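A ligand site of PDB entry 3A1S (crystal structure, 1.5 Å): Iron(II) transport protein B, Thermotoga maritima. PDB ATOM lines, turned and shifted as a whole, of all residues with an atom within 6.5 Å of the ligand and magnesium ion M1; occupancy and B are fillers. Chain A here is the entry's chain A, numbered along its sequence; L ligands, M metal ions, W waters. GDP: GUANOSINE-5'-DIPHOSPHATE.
N of Val 16 is in hydrogen-bond range of O1B of the ligand (3.0 Å).
The backbone NH (N) of Asn 15 sits at hydrogen-bond distance from an oxygen (O1B) of the ligand, 3.4 Å away.
A nitrogen (N1) of the ligand is in hydrogen-bond range of the side-chain carboxylate (OD1) of Asp 121 (2.8 Å).
OG1 of Thr 19 is in hydrogen-bond range of O2B of the ligand, at 2.7 Å.
An oxygen (O6) of the ligand sits at hydrogen-bond distance from the backbone NH (N) of Ala 119, 3.3 Å away.
N of Lys 18 lies within hydrogen-bond range of O1B of the ligand, 2.9 Å away.
N of Thr 19 is in hydrogen-bond range of O2B of the ligand.
The backbone NH of Gly 17 is in hydrogen-bond range of an oxygen (O3A) of the ligand, 3.0 Å away.
O6 of the ligand sits at hydrogen-bond distance from N of Ser 148 (2.8 Å).
An oxygen (O1A) of the ligand sits at hydrogen-bond distance from the backbone NH (N) of Ser 20.
O1A of the ligand sits at hydrogen-bond distance from OG of Ser 20 (2.6 Å).
The backbone carbonyl oxygen (O) of Ser 20 sits close to the side-chain hydroxyl (OG) of Ser 148, 3.3 Å away.
The backbone carbonyl oxygen of Thr 146 lies within hydrogen-bond range of the backbone NH of Ala 119, at 3.1 Å.
OG1 of Thr 118 sits at hydrogen-bond distance from OG1 of Thr 146, 2.9 Å away.
The side-chain hydroxyl of Ser 147 lies within hydrogen-bond range of the backbone NH of Val 149, at 3.1 Å.
OG of Ser 148 lies within hydrogen-bond range of N of Leu 21 (3.2 Å).
NZ of Lys 18 lies within salt-bridge range of OD1 of Asp 58, 2.6 Å away.
N of Thr 150 sits at hydrogen-bond distance from OG of Ser 147 (3.1 Å).
The side-chain carboxylate (OD1) of Asp 121 lies within hydrogen-bond range of the side-chain hydroxyl (OG) of Ser 147, at 2.7 Å.
Residues that only touch the ligand: Thr 118 (3.7 Å), Glu 122 (3.9 Å), Ser 147 (3.5 Å) and Val 149 (3.6 Å).
The nearest printed residue that does not touch the ligand is Cys 13 (4.1 Å).
No residue comes within 4 Å of magnesium ion M1.
Magnesium ion M1 is bound by O3B of the ligand, water W8, water W6 and water W11.
Magnesium ion M1 has four donor atoms within binding distance.
Water W9 lies within hydrogen-bond range of an oxygen (O1B) of the ligand, the backbone carbonyl oxygen of Cys 13 and the side-chain amino group of Lys 18.
Water W12 bridges O4' of the ligand and O of Asn 15.
Water W15 lies within hydrogen-bond range of an oxygen (O2B) of the ligand (2.8 Å), the side-chain amino group of Lys 18 (2.8 Å), the side-chain carboxylate of Asp 58 (3.2 Å) and the side-chain hydroxyl of Thr 19 (3.3 Å).
Water W5 lies within hydrogen-bond range of the side-chain hydroxyl (OG1) of Thr 118 (2.7 Å), a nitrogen (N7) of the ligand (2.8 Å), the backbone carbonyl oxygen (O) of Gly 17 (2.9 Å) and the side-chain hydroxyl (OG) of Ser 148 (2.9 Å).
Water W4 lies within hydrogen-bond range of the side-chain carboxylate (OE1) of Glu 122 (2.5 Å) and a nitrogen (N3) of the ligand (3.0 Å).
Water W1 bridges O4' of the ligand (3.3 Å) and OE1 of Glu 122 (3.4 Å).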
ATOM      1  N   GLY A  12     -28.633 -25.366  -5.975  1.00  0.00           N
ATOM      2  CA  GLY A  12     -27.903 -24.361  -6.726  1.00  0.00           C
ATOM      3  C   GLY A  12     -26.602 -24.865  -7.295  1.00  0.00           C
ATOM      4  O   GLY A  12     -26.103 -25.904  -6.888  1.00  0.00           O
ATOM      5  N   CYS A  13     -26.049 -24.108  -8.236  1.00  0.00           N
ATOM      6  CA  CYS A  13     -24.736 -24.426  -8.795  1.00  0.00           C
ATOM      7  C   CYS A  13     -23.686 -24.194  -7.726  1.00  0.00           C
ATOM      8  O   CYS A  13     -23.946 -23.522  -6.743  1.00  0.00           O
ATOM      9  CB  CYS A  13     -24.431 -23.536  -9.995  1.00  0.00           C
ATOM     10  SG  CYS A  13     -25.630 -23.645 -11.360  1.00  0.00           S
ATOM     11  N   PRO A  14     -22.488 -24.763  -7.917  1.00  0.00           N
ATOM     12  CA  PRO A  14     -21.410 -24.414  -6.987  1.00  0.00           C
ATOM     13  C   PRO A  14     -21.114 -22.913  -6.983  1.00  0.00           C
ATOM     14  O   PRO A  14     -21.242 -22.254  -8.021  1.00  0.00           O
ATOM     15  CB  PRO A  14     -20.210 -25.179  -7.553  1.00  0.00           C
ATOM     16  CG  PRO A  14     -20.830 -26.338  -8.294  1.00  0.00           C
ATOM     17  CD  PRO A  14     -22.070 -25.766  -8.917  1.00  0.00           C
ATOM     18  N   ASN A  15     -20.739 -22.382  -5.828  1.00  0.00           N
ATOM     19  CA  ASN A  15     -20.235 -21.012  -5.733  1.00  0.00           C
ATOM     20  C   ASN A  15     -21.263 -19.949  -6.102  1.00  0.00           C
ATOM     21  O   ASN A  15     -20.931 -18.941  -6.716  1.00  0.00           O
ATOM     22  CB  ASN A  15     -18.986 -20.842  -6.607  1.00  0.00           C
ATOM     23  CG  ASN A  15     -18.116 -19.694  -6.156  1.00  0.00           C
ATOM     24  OD1 ASN A  15     -17.927 -19.480  -4.964  1.00  0.00           O
ATOM     25  ND2 ASN A  15     -17.596 -18.937  -7.115  1.00  0.00           N
ATOM     26  N   VAL A  16     -22.525 -20.159  -5.723  1.00  0.00           N
ATOM     27  CA  VAL A  16     -23.553 -19.160  -5.981  1.00  0.00           C
ATOM     28  C   VAL A  16     -23.981 -18.396  -4.724  1.00  0.00           C
ATOM     29  O   VAL A  16     -24.699 -17.398  -4.819  1.00  0.00           O
ATOM     30  CB  VAL A  16     -24.819 -19.776  -6.628  1.00  0.00           C
ATOM     31  CG1 VAL A  16     -24.489 -20.376  -7.986  1.00  0.00           C
ATOM     32  CG2 VAL A  16     -25.478 -20.807  -5.698  1.00  0.00           C
ATOM     33  N   GLY A  17     -23.543 -18.857  -3.562  1.00  0.00           N
ATOM     34  CA  GLY A  17     -23.934 -18.236  -2.314  1.00  0.00           C
ATOM     35  C   GLY A  17     -24.837 -19.078  -1.434  1.00  0.00           C
ATOM     36  O   GLY A  17     -25.503 -18.553  -0.535  1.00  0.00           O
ATOM     37  N   LYS A  18     -24.878 -20.393  -1.683  1.00  0.00           N
ATOM     38  CA  LYS A  18     -25.736 -21.277  -0.904  1.00  0.00           C
ATOM     39  C   LYS A  18     -25.336 -21.347   0.570  1.00  0.00           C
ATOM     40  O   LYS A  18     -26.175 -21.197   1.458  1.00  0.00           O
ATOM     41  CB  LYS A  18     -25.773 -22.704  -1.494  1.00  0.00           C
ATOM     42  CG  LYS A  18     -26.657 -22.879  -2.707  1.00  0.00           C
ATOM     43  CD  LYS A  18     -27.366 -24.248  -2.685  1.00  0.00           C
ATOM     44  CE  LYS A  18     -26.467 -25.381  -3.159  1.00  0.00           C
ATOM     45  NZ  LYS A  18     -25.439 -25.760  -2.147  1.00  0.00           N
ATOM     46  N   THR A  19     -24.057 -21.612   0.825  1.00  0.00           N
ATOM     47  CA  THR A  19     -23.573 -21.709   2.201  1.00  0.00           C
ATOM     48  C   THR A  19     -23.873 -20.425   2.956  1.00  0.00           C
ATOM     49  O   THR A  19     -24.325 -20.468   4.098  1.00  0.00           O
ATOM     50  CB  THR A  19     -22.051 -21.969   2.252  1.00  0.00           C
ATOM     51  OG1 THR A  19     -21.756 -23.237   1.648  1.00  0.00           O
ATOM     52  CG2 THR A  19     -21.555 -21.977   3.709  1.00  0.00           C
ATOM     53  N   SER A  20     -23.630 -19.285   2.323  1.00  0.00           N
ATOM     54  CA  SER A  20     -23.843 -18.004   2.985  1.00  0.00           C
ATOM     55  C   SER A  20     -25.317 -17.775   3.330  1.00  0.00           C
ATOM     56  O   SER A  20     -25.636 -17.309   4.418  1.00  0.00           O
ATOM     57  CB  SER A  20     -23.279 -16.854   2.131  1.00  0.00           C
ATOM     58  OG  SER A  20     -21.887 -17.025   1.911  1.00  0.00           O
ATOM     59  N   LEU A  21     -26.207 -18.096   2.385  1.00  0.00           N
ATOM     60  CA  LEU A  21     -27.639 -17.950   2.627  1.00  0.00           C
ATOM     61  C   LEU A  21     -28.102 -18.923   3.717  1.00  0.00           C
ATOM     62  O   LEU A  21     -28.861 -18.550   4.615  1.00  0.00           O
ATOM     63  CB  LEU A  21     -28.437 -18.174   1.333  1.00  0.00           C
ATOM     64  CG  LEU A  21     -29.946 -17.937   1.408  1.00  0.00           C
ATOM     65  CD1 LEU A  21     -30.255 -16.523   1.900  1.00  0.00           C
ATOM     66  CD2 LEU A  21     -30.585 -18.177   0.051  1.00  0.00           C
ATOM     67  N   ASP A  58     -29.149 -28.311   2.742  1.00  0.00           N
ATOM     68  CA  ASP A  58     -28.310 -27.802   1.655  1.00  0.00           C
ATOM     69  C   ASP A  58     -27.897 -28.953   0.745  1.00  0.00           C
ATOM     70  O   ASP A  58     -27.273 -29.903   1.184  1.00  0.00           O
ATOM     71  CB  ASP A  58     -27.066 -27.080   2.200  1.00  0.00           C
ATOM     72  CG  ASP A  58     -26.389 -26.159   1.171  1.00  0.00           C
ATOM     73  OD1 ASP A  58     -26.888 -26.064   0.036  1.00  0.00           O
ATOM     74  OD2 ASP A  58     -25.358 -25.509   1.463  1.00  0.00           O
ATOM     75  N   VAL A  90     -31.017 -21.205  -5.312  1.00  0.00           N
ATOM     76  CA  VAL A  90     -30.159 -20.060  -5.005  1.00  0.00           C
ATOM     77  C   VAL A  90     -29.392 -19.703  -6.250  1.00  0.00           C
ATOM     78  O   VAL A  90     -28.613 -20.501  -6.763  1.00  0.00           O
ATOM     79  CB  VAL A  90     -29.164 -20.388  -3.875  1.00  0.00           C
ATOM     80  CG1 VAL A  90     -28.368 -19.151  -3.493  1.00  0.00           C
ATOM     81  CG2 VAL A  90     -29.897 -20.955  -2.661  1.00  0.00           C
ATOM     82  N   ASP A  92     -26.894 -16.922  -8.405  1.00  0.00           N
ATOM     83  CA  ASP A  92     -25.946 -15.817  -8.311  1.00  0.00           C
ATOM     84  C   ASP A  92     -26.469 -14.686  -9.188  1.00  0.00           C
ATOM     85  O   ASP A  92     -26.479 -14.803 -10.400  1.00  0.00           O
ATOM     86  CB  ASP A  92     -24.567 -16.264  -8.790  1.00  0.00           C
ATOM     87  CG  ASP A  92     -23.481 -15.255  -8.489  1.00  0.00           C
ATOM     88  OD1 ASP A  92     -23.811 -14.108  -8.111  1.00  0.00           O
ATOM     89  OD2 ASP A  92     -22.289 -15.602  -8.627  1.00  0.00           O
ATOM     90  N   THR A 118     -29.448 -14.148  -5.017  1.00  0.00           N
ATOM     91  CA  THR A 118     -28.618 -13.690  -3.914  1.00  0.00           C
ATOM     92  C   THR A 118     -27.407 -12.881  -4.382  1.00  0.00           C
ATOM     93  O   THR A 118     -27.180 -12.715  -5.590  1.00  0.00           O
ATOM     94  CB  THR A 118     -28.216 -14.848  -2.987  1.00  0.00           C
ATOM     95  OG1 THR A 118     -27.847 -14.326  -1.699  1.00  0.00           O
ATOM     96  CG2 THR A 118     -27.073 -15.683  -3.583  1.00  0.00           C
ATOM     97  N   ALA A 119     -26.649 -12.364  -3.418  1.00  0.00           N
ATOM     98  CA  ALA A 119     -25.574 -11.409  -3.684  1.00  0.00           C
ATOM     99  C   ALA A 119     -26.104 -10.182  -4.412  1.00  0.00           C
ATOM    100  O   ALA A 119     -25.403  -9.594  -5.223  1.00  0.00           O
ATOM    101  CB  ALA A 119     -24.461 -12.068  -4.496  1.00  0.00           C
ATOM    102  N   ILE A 120     -27.335  -9.803  -4.111  1.00  0.00           N
ATOM    103  CA  ILE A 120     -27.945  -8.648  -4.749  1.00  0.00           C
ATOM    104  C   ILE A 120     -27.171  -7.370  -4.438  1.00  0.00           C
ATOM    105  O   ILE A 120     -27.221  -6.396  -5.203  1.00  0.00           O
ATOM    106  CB  ILE A 120     -29.445  -8.483  -4.367  1.00  0.00           C
ATOM    107  CG1 ILE A 120     -30.189  -7.675  -5.438  1.00  0.00           C
ATOM    108  CG2 ILE A 120     -29.599  -7.896  -2.971  1.00  0.00           C
ATOM    109  CD1 ILE A 120     -30.368  -8.447  -6.729  1.00  0.00           C
ATOM    110  N   ASP A 121     -26.436  -7.365  -3.329  1.00  0.00           N
ATOM    111  CA  ASP A 121     -25.652  -6.190  -2.943  1.00  0.00           C
ATOM    112  C   ASP A 121     -24.462  -6.023  -3.879  1.00  0.00           C
ATOM    113  O   ASP A 121     -24.052  -4.899  -4.181  1.00  0.00           O
ATOM    114  CB  ASP A 121     -25.168  -6.304  -1.498  1.00  0.00           C
ATOM    115  CG  ASP A 121     -24.334  -7.555  -1.258  1.00  0.00           C
ATOM    116  OD1 ASP A 121     -24.870  -8.666  -1.394  1.00  0.00           O
ATOM    117  OD2 ASP A 121     -23.134  -7.401  -0.936  1.00  0.00           O
ATOM    118  N   GLU A 122     -23.925  -7.151  -4.340  1.00  0.00           N
ATOM    119  CA  GLU A 122     -22.822  -7.131  -5.283  1.00  0.00           C
ATOM    120  C   GLU A 122     -23.328  -6.748  -6.671  1.00  0.00           C
ATOM    121  O   GLU A 122     -22.694  -5.959  -7.377  1.00  0.00           O
ATOM    122  CB  GLU A 122     -22.110  -8.493  -5.331  1.00  0.00           C
ATOM    123  CG  GLU A 122     -20.916  -8.524  -6.271  1.00  0.00           C
ATOM    124  CD  GLU A 122     -20.195  -9.863  -6.260  1.00  0.00           C
ATOM    125  OE1 GLU A 122     -20.391 -10.626  -5.289  1.00  0.00           O
ATOM    126  OE2 GLU A 122     -19.440 -10.148  -7.207  1.00  0.00           O
ATOM    127  N   LYS A 125     -23.755  -2.945  -7.242  1.00  0.00           N
ATOM    128  CA  LYS A 125     -22.502  -2.212  -7.422  1.00  0.00           C
ATOM    129  C   LYS A 125     -22.061  -2.167  -8.878  1.00  0.00           C
ATOM    130  O   LYS A 125     -21.451  -1.198  -9.325  1.00  0.00           O
ATOM    131  CB  LYS A 125     -21.388  -2.817  -6.579  1.00  0.00           C
ATOM    132  CG  LYS A 125     -21.585  -2.687  -5.081  1.00  0.00           C
ATOM    133  CD  LYS A 125     -20.354  -3.193  -4.335  1.00  0.00           C
ATOM    134  CE  LYS A 125     -20.654  -3.479  -2.874  1.00  0.00           C
ATOM    135  NZ  LYS A 125     -21.096  -2.264  -2.137  1.00  0.00           N
ATOM    136  N   THR A 146     -31.950 -11.342  -2.456  1.00  0.00           N
ATOM    137  CA  THR A 146     -31.388 -11.513  -1.123  1.00  0.00           C
ATOM    138  C   THR A 146     -29.917 -11.111  -1.065  1.00  0.00           C
ATOM    139  O   THR A 146     -29.216 -11.145  -2.081  1.00  0.00           O
ATOM    140  CB  THR A 146     -31.495 -12.983  -0.624  1.00  0.00           C
ATOM    141  OG1 THR A 146     -30.737 -13.840  -1.477  1.00  0.00           O
ATOM    142  CG2 THR A 146     -32.948 -13.462  -0.578  1.00  0.00           C
ATOM    143  N   SER A 147     -29.469 -10.756   0.125  1.00  0.00           N
ATOM    144  CA  SER A 147     -28.044 -10.559   0.366  1.00  0.00           C
ATOM    145  C   SER A 147     -27.679 -11.134   1.721  1.00  0.00           C
ATOM    146  O   SER A 147     -28.289 -10.787   2.732  1.00  0.00           O
ATOM    147  CB  SER A 147     -27.686  -9.083   0.332  1.00  0.00           C
ATOM    148  OG  SER A 147     -26.348  -8.904   0.794  1.00  0.00           O
ATOM    149  N   SER A 148     -26.698 -12.022   1.745  1.00  0.00           N
ATOM    150  CA  SER A 148     -26.196 -12.576   2.997  1.00  0.00           C
ATOM    151  C   SER A 148     -25.263 -11.608   3.711  1.00  0.00           C
ATOM    152  O   SER A 148     -24.877 -11.841   4.852  1.00  0.00           O
ATOM    153  CB  SER A 148     -25.478 -13.896   2.745  1.00  0.00           C
ATOM    154  OG  SER A 148     -26.406 -14.879   2.331  1.00  0.00           O
ATOM    155  N   VAL A 149     -24.884 -10.539   3.029  1.00  0.00           N
ATOM    156  CA  VAL A 149     -24.019  -9.516   3.620  1.00  0.00           C
ATOM    157  C   VAL A 149     -24.834  -8.453   4.350  1.00  0.00           C
ATOM    158  O   VAL A 149     -24.548  -8.132   5.513  1.00  0.00           O
ATOM    159  CB  VAL A 149     -23.139  -8.844   2.554  1.00  0.00           C
ATOM    160  CG1 VAL A 149     -22.537  -7.544   3.080  1.00  0.00           C
ATOM    161  CG2 VAL A 149     -22.039  -9.802   2.094  1.00  0.00           C
ATOM    162  N   THR A 150     -25.859  -7.916   3.690  1.00  0.00           N
ATOM    163  CA  THR A 150     -26.644  -6.815   4.253  1.00  0.00           C
ATOM    164  C   THR A 150     -27.918  -7.287   4.951  1.00  0.00           C
ATOM    165  O   THR A 150     -28.483  -6.573   5.774  1.00  0.00           O
ATOM    166  CB  THR A 150     -27.068  -5.812   3.169  1.00  0.00           C
ATOM    167  OG1 THR A 150     -27.991  -6.433   2.281  1.00  0.00           O
ATOM    168  CG2 THR A 150     -25.848  -5.326   2.395  1.00  0.00           C
HETATM  169  PB  GDP L   1     -21.612 -21.763  -2.243  1.00  0.00           P
HETATM  170  O1B GDP L   1     -22.782 -21.754  -3.199  1.00  0.00           O
HETATM  171  O2B GDP L   1     -21.967 -22.429  -0.937  1.00  0.00           O
HETATM  172  O3B GDP L   1     -20.394 -22.372  -2.912  1.00  0.00           O
HETATM  173  O3A GDP L   1     -21.306 -20.190  -2.045  1.00  0.00           O
HETATM  174  PA  GDP L   1     -20.780 -19.366  -0.786  1.00  0.00           P
HETATM  175  O1A GDP L   1     -21.884 -19.013   0.170  1.00  0.00           O
HETATM  176  O2A GDP L   1     -19.611 -20.067  -0.108  1.00  0.00           O
HETATM  177  O5' GDP L   1     -20.341 -17.995  -1.480  1.00  0.00           O
HETATM  178  C5' GDP L   1     -19.390 -17.955  -2.544  1.00  0.00           C
HETATM  179  C4' GDP L   1     -18.805 -16.560  -2.606  1.00  0.00           C
HETATM  180  O4' GDP L   1     -19.894 -15.624  -2.733  1.00  0.00           O
HETATM  181  C3' GDP L   1     -18.088 -16.211  -1.329  1.00  0.00           C
HETATM  182  O3' GDP L   1     -17.007 -15.359  -1.684  1.00  0.00           O
HETATM  183  C2' GDP L   1     -19.109 -15.415  -0.545  1.00  0.00           C
HETATM  184  O2' GDP L   1     -18.522 -14.477   0.347  1.00  0.00           O
HETATM  185  C1' GDP L   1     -19.836 -14.694  -1.667  1.00  0.00           C
HETATM  186  N9  GDP L   1     -21.230 -14.411  -1.313  1.00  0.00           N
HETATM  187  C8  GDP L   1     -22.189 -15.288  -1.016  1.00  0.00           C
HETATM  188  N7  GDP L   1     -23.363 -14.655  -0.752  1.00  0.00           N
HETATM  189  C5  GDP L   1     -23.132 -13.337  -0.922  1.00  0.00           C
HETATM  190  C6  GDP L   1     -23.916 -12.094  -0.828  1.00  0.00           C
HETATM  191  O6  GDP L   1     -25.117 -12.176  -0.514  1.00  0.00           O
HETATM  192  N1  GDP L   1     -23.279 -10.943  -1.075  1.00  0.00           N
HETATM  193  C2  GDP L   1     -21.983 -10.859  -1.421  1.00  0.00           C
HETATM  194  N2  GDP L   1     -21.409  -9.669  -1.669  1.00  0.00           N
HETATM  195  N3  GDP L   1     -21.204 -11.963  -1.526  1.00  0.00           N
HETATM  196  C4  GDP L   1     -21.727 -13.182  -1.298  1.00  0.00           C
HETATM  197 MG    MG M   1     -18.590 -23.292  -2.461  1.00  0.00          MG
HETATM  198 MG    MG M   2     -20.558 -14.595  -6.826  1.00  0.00          MG
HETATM  199  O   HOH W   1     -18.944 -13.737  -5.241  1.00  0.00           O
HETATM  200  O   HOH W   2     -15.238 -15.079   0.351  1.00  0.00           O
HETATM  201  O   HOH W   3     -18.597 -21.178   2.161  1.00  0.00           O
HETATM  202  O   HOH W   4     -19.051 -11.832  -3.573  1.00  0.00           O
HETATM  203  O   HOH W   5     -25.906 -15.730  -0.355  1.00  0.00           O
HETATM  204  O   HOH W   6     -17.505 -21.897  -3.779  1.00  0.00           O
HETATM  205  O   HOH W   7     -17.319 -11.778  -0.186  1.00  0.00           O
HETATM  206  O   HOH W   8     -18.875 -24.626  -4.114  1.00  0.00           O
HETATM  207  O   HOH W   9     -23.429 -24.223  -4.075  1.00  0.00           O
HETATM  208  O   HOH W  10     -18.470  -8.702  -1.930  1.00  0.00           O
HETATM  209  O   HOH W  11     -18.587 -22.267  -0.474  1.00  0.00           O
HETATM  210  O   HOH W  12     -21.223 -16.140  -5.042  1.00  0.00           O
HETATM  211  O   HOH W  13     -18.001 -15.709   2.949  1.00  0.00           O
HETATM  212  O   HOH W  14     -15.456 -15.395  -3.899  1.00  0.00           O
HETATM  213  O   HOH W  15     -23.183 -24.924  -0.744  1.00  0.00           O
